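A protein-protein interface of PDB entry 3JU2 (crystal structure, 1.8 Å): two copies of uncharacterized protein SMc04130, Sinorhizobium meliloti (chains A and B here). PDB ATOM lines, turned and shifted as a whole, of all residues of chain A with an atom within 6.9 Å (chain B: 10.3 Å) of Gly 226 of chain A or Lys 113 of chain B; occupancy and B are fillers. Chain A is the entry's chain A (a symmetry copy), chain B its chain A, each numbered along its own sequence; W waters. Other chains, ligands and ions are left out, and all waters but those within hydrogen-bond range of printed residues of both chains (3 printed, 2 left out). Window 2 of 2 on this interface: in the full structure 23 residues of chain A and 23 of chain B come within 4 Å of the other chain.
The side-chain amino group of Lys 113 of chain B is in hydrogen-bond range of the backbone carbonyl oxygen of Gly 226 of chain A, 2.9 Å away.
The backbone NH (N) of Leu 108 of chain B is in hydrogen-bond range of the backbone carbonyl oxygen (O) of Ala 151 of chain B (2.8 Å). N of Gly 226 of chain A is in hydrogen-bond range of OD1 of Asp 208 of chain A (2.9 Å). The side-chain carboxylate (OD2) of Asp 208 of chain A sits at hydrogen-bond distance from the backbone NH (N) of Ile 228 of chain A, 2.9 Å away. N of Val 227 of chain A lies within hydrogen-bond range of O of Trp 209 of chain A, at 3.0 Å. The side-chain carboxylate of Asp 208 of chain A sits at hydrogen-bond distance from the backbone NH of Val 227 of chain A (3.1 Å).
CZ3 of Trp 183 of chain A touches CD1 of Ile 115 of chain B, at 3.5 Å. Ala 150 of chain B touches Trp 183 of chain A (CB to CH2, 3.9 Å). Trp 183 of chain A touches Ala 151 of chain B (CH2 to CB, 3.7 Å). Ala 151 of chain B touches Trp 209 of chain A (CB to CD1, 3.7 Å). Val 211 of chain A touches Ala 151 of chain B (CG2 to CB, 3.6 Å). Val 227 of chain A touches Leu 108 of chain B. Val 227 of chain A touches Lys 113 of chain B (O to CB, 3.4 Å). Val 227 of chain A touches Ala 151 of chain B. Ile 228 of chain A touches Lys 113 of chain B (O to CD, 3.6 Å). CB of Asp 229 of chain A touches O of Lys 113 of chain B, at 3.7 Å.
Of the printed residues of chain B, Trp 183 of chain A touches Ile 115 (3.5 Å), Ala 150 (3.9 Å) and Ala 151 (3.7 Å). Asp 208 of chain A touches none of the printed residues of chain B. No residue of chain B comes within 4 Å of Asp 225 of chain A. Gly 226 of chain A touches just one residue of chain B: Lys 113. Val 227 of chain A touches just these residues of chain B: Leu 108 (3.7 Å), Lys 113 (3.4 Å) and Ala 151 (3.7 Å). Lys 113 of chain B touches just these residues of chain A: Gly 226, Val 227, Ile 228 and Asp 229. Of the printed residues of chain A, Ile 115 of chain B touches Trp 183 (3.5 Å). The nearest residue of chain A that does not touch Lys 113 of chain B is Gly 224 of chain A (4.3 Å). The nearest printed residue of chain A that does not touch Ala 151 of chain B is Leu 210 of chain A (5.4 Å).
Along chain A the printed residues that touch a printed residue of chain B span positions 183 to 229. Among the printed residues, 11 pairs touch across the chains. Among the printed residues, no Asp or Glu carboxylate lies within 4 Å of a Lys or Arg side-chain nitrogen of the other chain.
No position is printed for both chains. Of the 11 pairs that touch across the chains among the printed residues, none has its exchanged pair printed and touching as well.
Water W1 lies within hydrogen-bond range of the backbone carbonyl oxygen of Gly 224 of chain A and the side-chain amino group of Lys 113 of chain B. Water W3 lies within hydrogen-bond range of O of Trp 183 of chain A (2.7 Å) and NH2 of Arg 119 of chain B (3.1 Å). Water W2 lies within hydrogen-bond range of the backbone carbonyl oxygen of Val 227 of chain A (2.8 Å) and the backbone carbonyl oxygen of Lys 113 of chain B (2.8 Å).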
ATOM      1  N   TRP A 183      -3.414   2.261  23.965  1.00  0.00           N
ATOM      2  CA  TRP A 183      -1.943   2.392  24.080  1.00  0.00           C
ATOM      3  C   TRP A 183      -1.478   3.120  25.353  1.00  0.00           C
ATOM      4  O   TRP A 183      -0.429   2.797  25.892  1.00  0.00           O
ATOM      5  CB  TRP A 183      -1.323   3.080  22.823  1.00  0.00           C
ATOM      6  CG  TRP A 183      -1.554   4.567  22.832  1.00  0.00           C
ATOM      7  CD1 TRP A 183      -2.676   5.240  22.405  1.00  0.00           C
ATOM      8  CD2 TRP A 183      -0.672   5.551  23.364  1.00  0.00           C
ATOM      9  NE1 TRP A 183      -2.526   6.588  22.632  1.00  0.00           N
ATOM     10  CE2 TRP A 183      -1.311   6.805  23.227  1.00  0.00           C
ATOM     11  CE3 TRP A 183       0.606   5.496  23.942  1.00  0.00           C
ATOM     12  CZ2 TRP A 183      -0.722   7.987  23.656  1.00  0.00           C
ATOM     13  CZ3 TRP A 183       1.201   6.665  24.353  1.00  0.00           C
ATOM     14  CH2 TRP A 183       0.531   7.906  24.220  1.00  0.00           C
ATOM     15  N   ASP A 208      -1.721   4.706  14.543  1.00  0.00           N
ATOM     16  CA  ASP A 208      -0.798   5.378  15.419  1.00  0.00           C
ATOM     17  C   ASP A 208      -1.403   6.613  16.035  1.00  0.00           C
ATOM     18  O   ASP A 208      -2.331   7.159  15.538  1.00  0.00           O
ATOM     19  CB  ASP A 208       0.498   5.728  14.698  1.00  0.00           C
ATOM     20  CG  ASP A 208       1.740   5.525  15.551  1.00  0.00           C
ATOM     21  OD1 ASP A 208       2.790   5.311  14.975  1.00  0.00           O
ATOM     22  OD2 ASP A 208       1.687   5.604  16.763  1.00  0.00           O
ATOM     23  N   TRP A 209      -0.841   7.011  17.145  1.00  0.00           N
ATOM     24  CA  TRP A 209      -1.238   8.212  17.863  1.00  0.00           C
ATOM     25  C   TRP A 209      -0.267   9.319  17.467  1.00  0.00           C
ATOM     26  O   TRP A 209       0.917   9.315  17.837  1.00  0.00           O
ATOM     27  CB  TRP A 209      -1.185   7.991  19.393  1.00  0.00           C
ATOM     28  CG  TRP A 209      -1.683   9.177  20.157  1.00  0.00           C
ATOM     29  CD1 TRP A 209      -0.955  10.257  20.563  1.00  0.00           C
ATOM     30  CD2 TRP A 209      -3.038   9.426  20.563  1.00  0.00           C
ATOM     31  NE1 TRP A 209      -1.771  11.160  21.204  1.00  0.00           N
ATOM     32  CE2 TRP A 209      -3.051  10.676  21.222  1.00  0.00           C
ATOM     33  CE3 TRP A 209      -4.239   8.715  20.426  1.00  0.00           C
ATOM     34  CZ2 TRP A 209      -4.229  11.244  21.770  1.00  0.00           C
ATOM     35  CZ3 TRP A 209      -5.416   9.268  20.972  1.00  0.00           C
ATOM     36  CH2 TRP A 209      -5.396  10.531  21.622  1.00  0.00           C
ATOM     37  N   LEU A 210      -0.789  10.310  16.760  1.00  0.00           N
ATOM     38  CA  LEU A 210       0.037  11.422  16.304  1.00  0.00           C
ATOM     39  C   LEU A 210       0.339  12.430  17.397  1.00  0.00           C
ATOM     40  O   LEU A 210      -0.470  12.649  18.328  1.00  0.00           O
ATOM     41  CB  LEU A 210      -0.636  12.114  15.112  1.00  0.00           C
ATOM     42  CG  LEU A 210      -0.840  11.205  13.904  1.00  0.00           C
ATOM     43  CD1 LEU A 210      -1.606  11.926  12.777  1.00  0.00           C
ATOM     44  CD2 LEU A 210       0.521  10.668  13.386  1.00  0.00           C
ATOM     45  N   VAL A 211       1.521  13.030  17.313  1.00  0.00           N
ATOM     46  CA  VAL A 211       1.829  14.201  18.143  1.00  0.00           C
ATOM     47  C   VAL A 211       2.172  15.432  17.266  1.00  0.00           C
ATOM     48  O   VAL A 211       3.186  15.415  16.580  1.00  0.00           O
ATOM     49  CB  VAL A 211       3.001  13.922  19.148  1.00  0.00           C
ATOM     50  CG1 VAL A 211       3.305  15.151  19.982  1.00  0.00           C
ATOM     51  CG2 VAL A 211       2.643  12.771  20.070  1.00  0.00           C
ATOM     52  N   GLY A 221      -3.127   8.286  13.006  1.00  0.00           N
ATOM     53  CA  GLY A 221      -1.925   8.160  12.186  1.00  0.00           C
ATOM     54  C   GLY A 221      -1.745   6.839  11.468  1.00  0.00           C
ATOM     55  O   GLY A 221      -2.303   5.797  11.865  1.00  0.00           O
ATOM     56  N   MET A 222      -0.957   6.889  10.397  1.00  0.00           N
ATOM     57  CA  MET A 222      -0.395   5.695   9.795  1.00  0.00           C
ATOM     58  C   MET A 222       0.664   5.158  10.755  1.00  0.00           C
ATOM     59  O   MET A 222       1.376   5.925  11.383  1.00  0.00           O
ATOM     60  CB  MET A 222       0.255   6.037   8.438  1.00  0.00           C
ATOM     61  CG  MET A 222       0.867   4.829   7.664  1.00  0.00           C
ATOM     62  SD  MET A 222      -0.089   3.482   7.096  1.00  0.00           S
ATOM     63  CE  MET A 222      -1.079   4.310   5.818  1.00  0.00           C
ATOM     64  N   MET A 223       0.739   3.844  10.851  1.00  0.00           N
ATOM     65  CA  MET A 223       1.742   3.156  11.677  1.00  0.00           C
ATOM     66  C   MET A 223       3.140   3.709  11.435  1.00  0.00           C
ATOM     67  O   MET A 223       3.592   3.788  10.291  1.00  0.00           O
ATOM     68  CB  MET A 223       1.679   1.649  11.406  1.00  0.00           C
ATOM     69  CG  MET A 223       0.331   0.983  11.717  1.00  0.00           C
ATOM     70  SD  MET A 223      -1.008   1.028  10.491  1.00  0.00           S
ATOM     71  CE  MET A 223      -0.136   0.322   9.049  1.00  0.00           C
ATOM     72  N   GLY A 224       3.800   4.158  12.500  1.00  0.00           N
ATOM     73  CA  GLY A 224       5.147   4.728  12.388  1.00  0.00           C
ATOM     74  C   GLY A 224       5.214   6.241  12.335  1.00  0.00           C
ATOM     75  O   GLY A 224       6.260   6.827  12.610  1.00  0.00           O
ATOM     76  N   ASP A 225       4.099   6.885  11.984  1.00  0.00           N
ATOM     77  CA  ASP A 225       4.049   8.341  11.973  1.00  0.00           C
ATOM     78  C   ASP A 225       3.825   8.907  13.374  1.00  0.00           C
ATOM     79  O   ASP A 225       4.025  10.092  13.608  1.00  0.00           O
ATOM     80  CB  ASP A 225       2.916   8.825  11.054  1.00  0.00           C
ATOM     81  CG  ASP A 225       3.308   8.809   9.575  1.00  0.00           C
ATOM     82  OD1 ASP A 225       4.429   8.355   9.250  1.00  0.00           O
ATOM     83  OD2 ASP A 225       2.501   9.272   8.745  1.00  0.00           O
ATOM     84  N   GLY A 226       3.410   8.049  14.306  1.00  0.00           N
ATOM     85  CA  GLY A 226       3.136   8.511  15.656  1.00  0.00           C
ATOM     86  C   GLY A 226       4.076   8.000  16.729  1.00  0.00           C
ATOM     87  O   GLY A 226       5.265   7.760  16.485  1.00  0.00           O
ATOM     88  N   VAL A 227       3.540   7.838  17.938  1.00  0.00           N
ATOM     89  CA  VAL A 227       4.384   7.555  19.103  1.00  0.00           C
ATOM     90  C   VAL A 227       4.085   6.224  19.811  1.00  0.00           C
ATOM     91  O   VAL A 227       4.677   5.939  20.854  1.00  0.00           O
ATOM     92  CB  VAL A 227       4.354   8.714  20.132  1.00  0.00           C
ATOM     93  CG1 VAL A 227       4.981   9.979  19.542  1.00  0.00           C
ATOM     94  CG2 VAL A 227       2.936   8.976  20.643  1.00  0.00           C
ATOM     95  N   ILE A 228       3.195   5.411  19.248  1.00  0.00           N
ATOM     96  CA  ILE A 228       2.855   4.128  19.882  1.00  0.00           C
ATOM     97  C   ILE A 228       3.972   3.100  19.648  1.00  0.00           C
ATOM     98  O   ILE A 228       4.450   2.948  18.521  1.00  0.00           O
ATOM     99  CB  ILE A 228       1.524   3.572  19.356  1.00  0.00           C
ATOM    100  CG1 ILE A 228       0.374   4.558  19.648  1.00  0.00           C
ATOM    101  CG2 ILE A 228       1.212   2.210  19.964  1.00  0.00           C
ATOM    102  CD1 ILE A 228      -0.957   4.052  19.132  1.00  0.00           C
ATOM    103  N   ASP A 229       4.400   2.410  20.710  1.00  0.00           N
ATOM    104  CA  ASP A 229       5.272   1.225  20.550  1.00  0.00           C
ATOM    105  C   ASP A 229       4.515   0.021  20.003  1.00  0.00           C
ATOM    106  O   ASP A 229       4.157  -0.904  20.744  1.00  0.00           O
ATOM    107  CB  ASP A 229       5.987   0.895  21.877  1.00  0.00           C
ATOM    108  CG  ASP A 229       7.013  -0.247  21.745  1.00  0.00           C
ATOM    109  OD1 ASP A 229       7.256  -0.765  20.632  1.00  0.00           O
ATOM    110  OD2 ASP A 229       7.554  -0.651  22.790  1.00  0.00           O
ATOM    111  N   LEU A 230       4.295   0.021  18.687  1.00  0.00           N
ATOM    112  CA  LEU A 230       3.475  -0.981  18.026  1.00  0.00           C
ATOM    113  C   LEU A 230       4.064  -2.389  18.127  1.00  0.00           C
ATOM    114  O   LEU A 230       3.342  -3.370  18.362  1.00  0.00           O
ATOM    115  CB  LEU A 230       3.230  -0.588  16.535  1.00  0.00           C
ATOM    116  CG  LEU A 230       2.408   0.697  16.335  1.00  0.00           C
ATOM    117  CD1 LEU A 230       2.551   1.309  14.937  1.00  0.00           C
ATOM    118  CD2 LEU A 230       0.952   0.409  16.625  1.00  0.00           C
ATOM    119  N   ARG A 271       4.636  -0.048   5.949  1.00  0.00           N
ATOM    120  CA  ARG A 271       4.719   0.195   7.389  1.00  0.00           C
ATOM    121  C   ARG A 271       4.518  -1.090   8.180  1.00  0.00           C
ATOM    122  O   ARG A 271       5.168  -1.287   9.194  1.00  0.00           O
ATOM    123  CB  ARG A 271       3.682   1.230   7.819  1.00  0.00           C
ATOM    124  CG  ARG A 271       3.849   2.575   7.158  1.00  0.00           C
ATOM    125  CD  ARG A 271       5.248   3.148   7.352  1.00  0.00           C
ATOM    126  NE  ARG A 271       5.378   4.460   6.723  1.00  0.00           N
ATOM    127  CZ  ARG A 271       5.116   5.620   7.323  1.00  0.00           C
ATOM    128  NH1 ARG A 271       4.705   5.660   8.585  1.00  0.00           N
ATOM    129  NH2 ARG A 271       5.266   6.751   6.657  1.00  0.00           N
ATOM    130  N   GLY B 107       4.985  14.526  29.134  1.00  0.00           N
ATOM    131  CA  GLY B 107       4.728  13.398  28.226  1.00  0.00           C
ATOM    132  C   GLY B 107       6.008  12.698  27.809  1.00  0.00           C
ATOM    133  O   GLY B 107       7.011  12.718  28.544  1.00  0.00           O
ATOM    134  N   LEU B 108       5.973  12.059  26.644  1.00  0.00           N
ATOM    135  CA  LEU B 108       7.147  11.348  26.114  1.00  0.00           C
ATOM    136  C   LEU B 108       8.310  12.294  25.834  1.00  0.00           C
ATOM    137  O   LEU B 108       8.100  13.389  25.289  1.00  0.00           O
ATOM    138  CB  LEU B 108       6.790  10.588  24.837  1.00  0.00           C
ATOM    139  CG  LEU B 108       5.914   9.367  25.041  1.00  0.00           C
ATOM    140  CD1 LEU B 108       5.215   8.995  23.753  1.00  0.00           C
ATOM    141  CD2 LEU B 108       6.773   8.222  25.554  1.00  0.00           C
ATOM    142  N   PRO B 109       9.540  11.898  26.235  1.00  0.00           N
ATOM    143  CA  PRO B 109      10.668  12.789  25.970  1.00  0.00           C
ATOM    144  C   PRO B 109      11.146  12.656  24.526  1.00  0.00           C
ATOM    145  O   PRO B 109      11.030  11.574  23.941  1.00  0.00           O
ATOM    146  CB  PRO B 109      11.733  12.301  26.943  1.00  0.00           C
ATOM    147  CG  PRO B 109      11.443  10.858  27.148  1.00  0.00           C
ATOM    148  CD  PRO B 109       9.956  10.664  26.927  1.00  0.00           C
ATOM    149  N   GLY B 110      11.655  13.752  23.961  1.00  0.00           N
ATOM    150  CA  GLY B 110      12.155  13.772  22.579  1.00  0.00           C
ATOM    151  C   GLY B 110      11.270  12.995  21.626  1.00  0.00           C
ATOM    152  O   GLY B 110      10.067  13.256  21.532  1.00  0.00           O
ATOM    153  N   GLY B 111      11.850  12.000  20.965  1.00  0.00           N
ATOM    154  CA  GLY B 111      11.083  11.163  20.045  1.00  0.00           C
ATOM    155  C   GLY B 111      10.880   9.728  20.510  1.00  0.00           C
ATOM    156  O   GLY B 111      10.665   8.838  19.685  1.00  0.00           O
ATOM    157  N   SER B 112      10.954   9.507  21.828  1.00  0.00           N
ATOM    158  CA  SER B 112      10.731   8.187  22.431  1.00  0.00           C
ATOM    159  C   SER B 112       9.308   7.677  22.233  1.00  0.00           C
ATOM    160  O   SER B 112       8.350   8.461  22.223  1.00  0.00           O
ATOM    161  CB  SER B 112      11.037   8.219  23.941  1.00  0.00           C
ATOM    162  OG  SER B 112      10.916   6.918  24.477  1.00  0.00           O
ATOM    163  N   LYS B 113       9.189   6.360  22.074  1.00  0.00           N
ATOM    164  CA  LYS B 113       7.912   5.655  22.097  1.00  0.00           C
ATOM    165  C   LYS B 113       7.771   4.839  23.410  1.00  0.00           C
ATOM    166  O   LYS B 113       6.829   4.065  23.570  1.00  0.00           O
ATOM    167  CB  LYS B 113       7.817   4.696  20.906  1.00  0.00           C
ATOM    168  CG  LYS B 113       7.948   5.357  19.511  1.00  0.00           C
ATOM    169  CD  LYS B 113       7.761   4.284  18.438  1.00  0.00           C
ATOM    170  CE  LYS B 113       8.221   4.761  17.062  1.00  0.00           C
ATOM    171  NZ  LYS B 113       7.554   6.036  16.653  1.00  0.00           N
ATOM    172  N   ASN B 114       8.735   4.998  24.308  1.00  0.00           N
ATOM    173  CA  ASN B 114       8.778   4.230  25.566  1.00  0.00           C
ATOM    174  C   ASN B 114       8.041   4.955  26.701  1.00  0.00           C
ATOM    175  O   ASN B 114       8.632   5.746  27.479  1.00  0.00           O
ATOM    176  CB  ASN B 114      10.230   3.914  25.966  1.00  0.00           C
ATOM    177  CG  ASN B 114      10.328   2.731  26.925  1.00  0.00           C
ATOM    178  OD1 ASN B 114       9.354   2.358  27.591  1.00  0.00           O
ATOM    179  ND2 ASN B 114      11.513   2.136  26.998  1.00  0.00           N
ATOM    180  N   ILE B 115       6.743   4.685  26.771  1.00  0.00           N
ATOM    181  CA  ILE B 115       5.882   5.336  27.754  1.00  0.00           C
ATOM    182  C   ILE B 115       6.155   4.798  29.164  1.00  0.00           C
ATOM    183  O   ILE B 115       6.116   5.562  30.126  1.00  0.00           O
ATOM    184  CB  ILE B 115       4.360   5.294  27.340  1.00  0.00           C
ATOM    185  CG1 ILE B 115       3.529   6.208  28.252  1.00  0.00           C
ATOM    186  CG2 ILE B 115       3.832   3.869  27.276  1.00  0.00           C
ATOM    187  CD1 ILE B 115       2.221   6.676  27.660  1.00  0.00           C
ATOM    188  N   ASP B 116       6.485   3.502  29.263  1.00  0.00           N
ATOM    189  CA  ASP B 116       6.944   2.884  30.548  1.00  0.00           C
ATOM    190  C   ASP B 116       8.163   3.614  31.119  1.00  0.00           C
ATOM    191  O   ASP B 116       8.201   3.976  32.313  1.00  0.00           O
ATOM    192  CB  ASP B 116       7.247   1.389  30.365  1.00  0.00           C
ATOM    193  CG  ASP B 116       6.004   0.560  30.048  1.00  0.00           C
ATOM    194  OD1 ASP B 116       4.886   1.121  29.944  1.00  0.00           O
ATOM    195  OD2 ASP B 116       6.145  -0.676  29.909  1.00  0.00           O
ATOM    196  N   ALA B 117       9.151   3.866  30.262  1.00  0.00           N
ATOM    197  CA  ALA B 117      10.334   4.606  30.663  1.00  0.00           C
ATOM    198  C   ALA B 117      10.025   6.040  31.061  1.00  0.00           C
ATOM    199  O   ALA B 117      10.568   6.518  32.045  1.00  0.00           O
ATOM    200  CB  ALA B 117      11.424   4.569  29.570  1.00  0.00           C
ATOM    201  N   ALA B 118       9.146   6.728  30.320  1.00  0.00           N
ATOM    202  CA  ALA B 118       8.794   8.098  30.667  1.00  0.00           C
ATOM    203  C   ALA B 118       8.117   8.143  32.046  1.00  0.00           C
ATOM    204  O   ALA B 118       8.377   9.050  32.858  1.00  0.00           O
ATOM    205  CB  ALA B 118       7.881   8.726  29.581  1.00  0.00           C
ATOM    206  N   ARG B 119       7.272   7.146  32.306  1.00  0.00           N
ATOM    207  CA  ARG B 119       6.592   7.023  33.596  1.00  0.00           C
ATOM    208  C   ARG B 119       7.577   6.766  34.754  1.00  0.00           C
ATOM    209  O   ARG B 119       7.440   7.353  35.822  1.00  0.00           O
ATOM    210  CB  ARG B 119       5.506   5.967  33.507  1.00  0.00           C
ATOM    211  CG  ARG B 119       4.251   6.522  32.820  1.00  0.00           C
ATOM    212  CD  ARG B 119       3.289   5.479  32.315  1.00  0.00           C
ATOM    213  NE  ARG B 119       2.124   6.151  31.744  1.00  0.00           N
ATOM    214  CZ  ARG B 119       1.215   5.595  30.940  1.00  0.00           C
ATOM    215  NH1 ARG B 119       0.193   6.335  30.506  1.00  0.00           N
ATOM    216  NH2 ARG B 119       1.311   4.328  30.559  1.00  0.00           N
ATOM    217  N   MET B 121      10.633   7.857  34.728  1.00  0.00           N
ATOM    218  CA  MET B 121      11.233   9.196  34.892  1.00  0.00           C
ATOM    219  C   MET B 121      10.396  10.140  35.770  1.00  0.00           C
ATOM    220  O   MET B 121      10.953  10.946  36.508  1.00  0.00           O
ATOM    221  CB  MET B 121      11.468   9.906  33.532  1.00  0.00           C
ATOM    222  CG  MET B 121      12.446   9.236  32.569  1.00  0.00           C
ATOM    223  SD  MET B 121      12.561   9.993  30.904  1.00  0.00           S
ATOM    224  CE  MET B 121      13.673   8.795  30.169  1.00  0.00           C
ATOM    225  N   ALA B 150      -1.643  11.937  27.117  1.00  0.00           N
ATOM    226  CA  ALA B 150      -0.585  10.996  27.543  1.00  0.00           C
ATOM    227  C   ALA B 150       0.746  11.175  26.811  1.00  0.00           C
ATOM    228  O   ALA B 150       1.810  11.151  27.444  1.00  0.00           O
ATOM    229  CB  ALA B 150      -1.079   9.545  27.419  1.00  0.00           C
ATOM    230  N   ALA B 151       0.680  11.382  25.495  1.00  0.00           N
ATOM    231  CA  ALA B 151       1.887  11.458  24.640  1.00  0.00           C
ATOM    232  C   ALA B 151       2.726  12.721  24.844  1.00  0.00           C
ATOM    233  O   ALA B 151       3.953  12.666  24.784  1.00  0.00           O
ATOM    234  CB  ALA B 151       1.487  11.322  23.149  1.00  0.00           C
ATOM    235  N   CYS B 155       1.974  11.769  31.357  1.00  0.00           N
ATOM    236  CA  CYS B 155       1.807  10.338  31.240  1.00  0.00           C
ATOM    237  C   CYS B 155       1.381   9.725  32.596  1.00  0.00           C
ATOM    238  O   CYS B 155       1.448   8.516  32.766  1.00  0.00           O
ATOM    239  CB  CYS B 155       3.087   9.661  30.708  1.00  0.00           C
ATOM    240  SG  CYS B 155       4.614   9.988  31.655  1.00  0.00           S
HETATM  241  O   HOH W   1       8.487   6.020  13.933  1.00  0.00           O
HETATM  242  O   HOH W   2       4.219   5.186  23.483  1.00  0.00           O
HETATM  243  O   HOH W   3       0.554   2.280  28.393  1.00  0.00           O
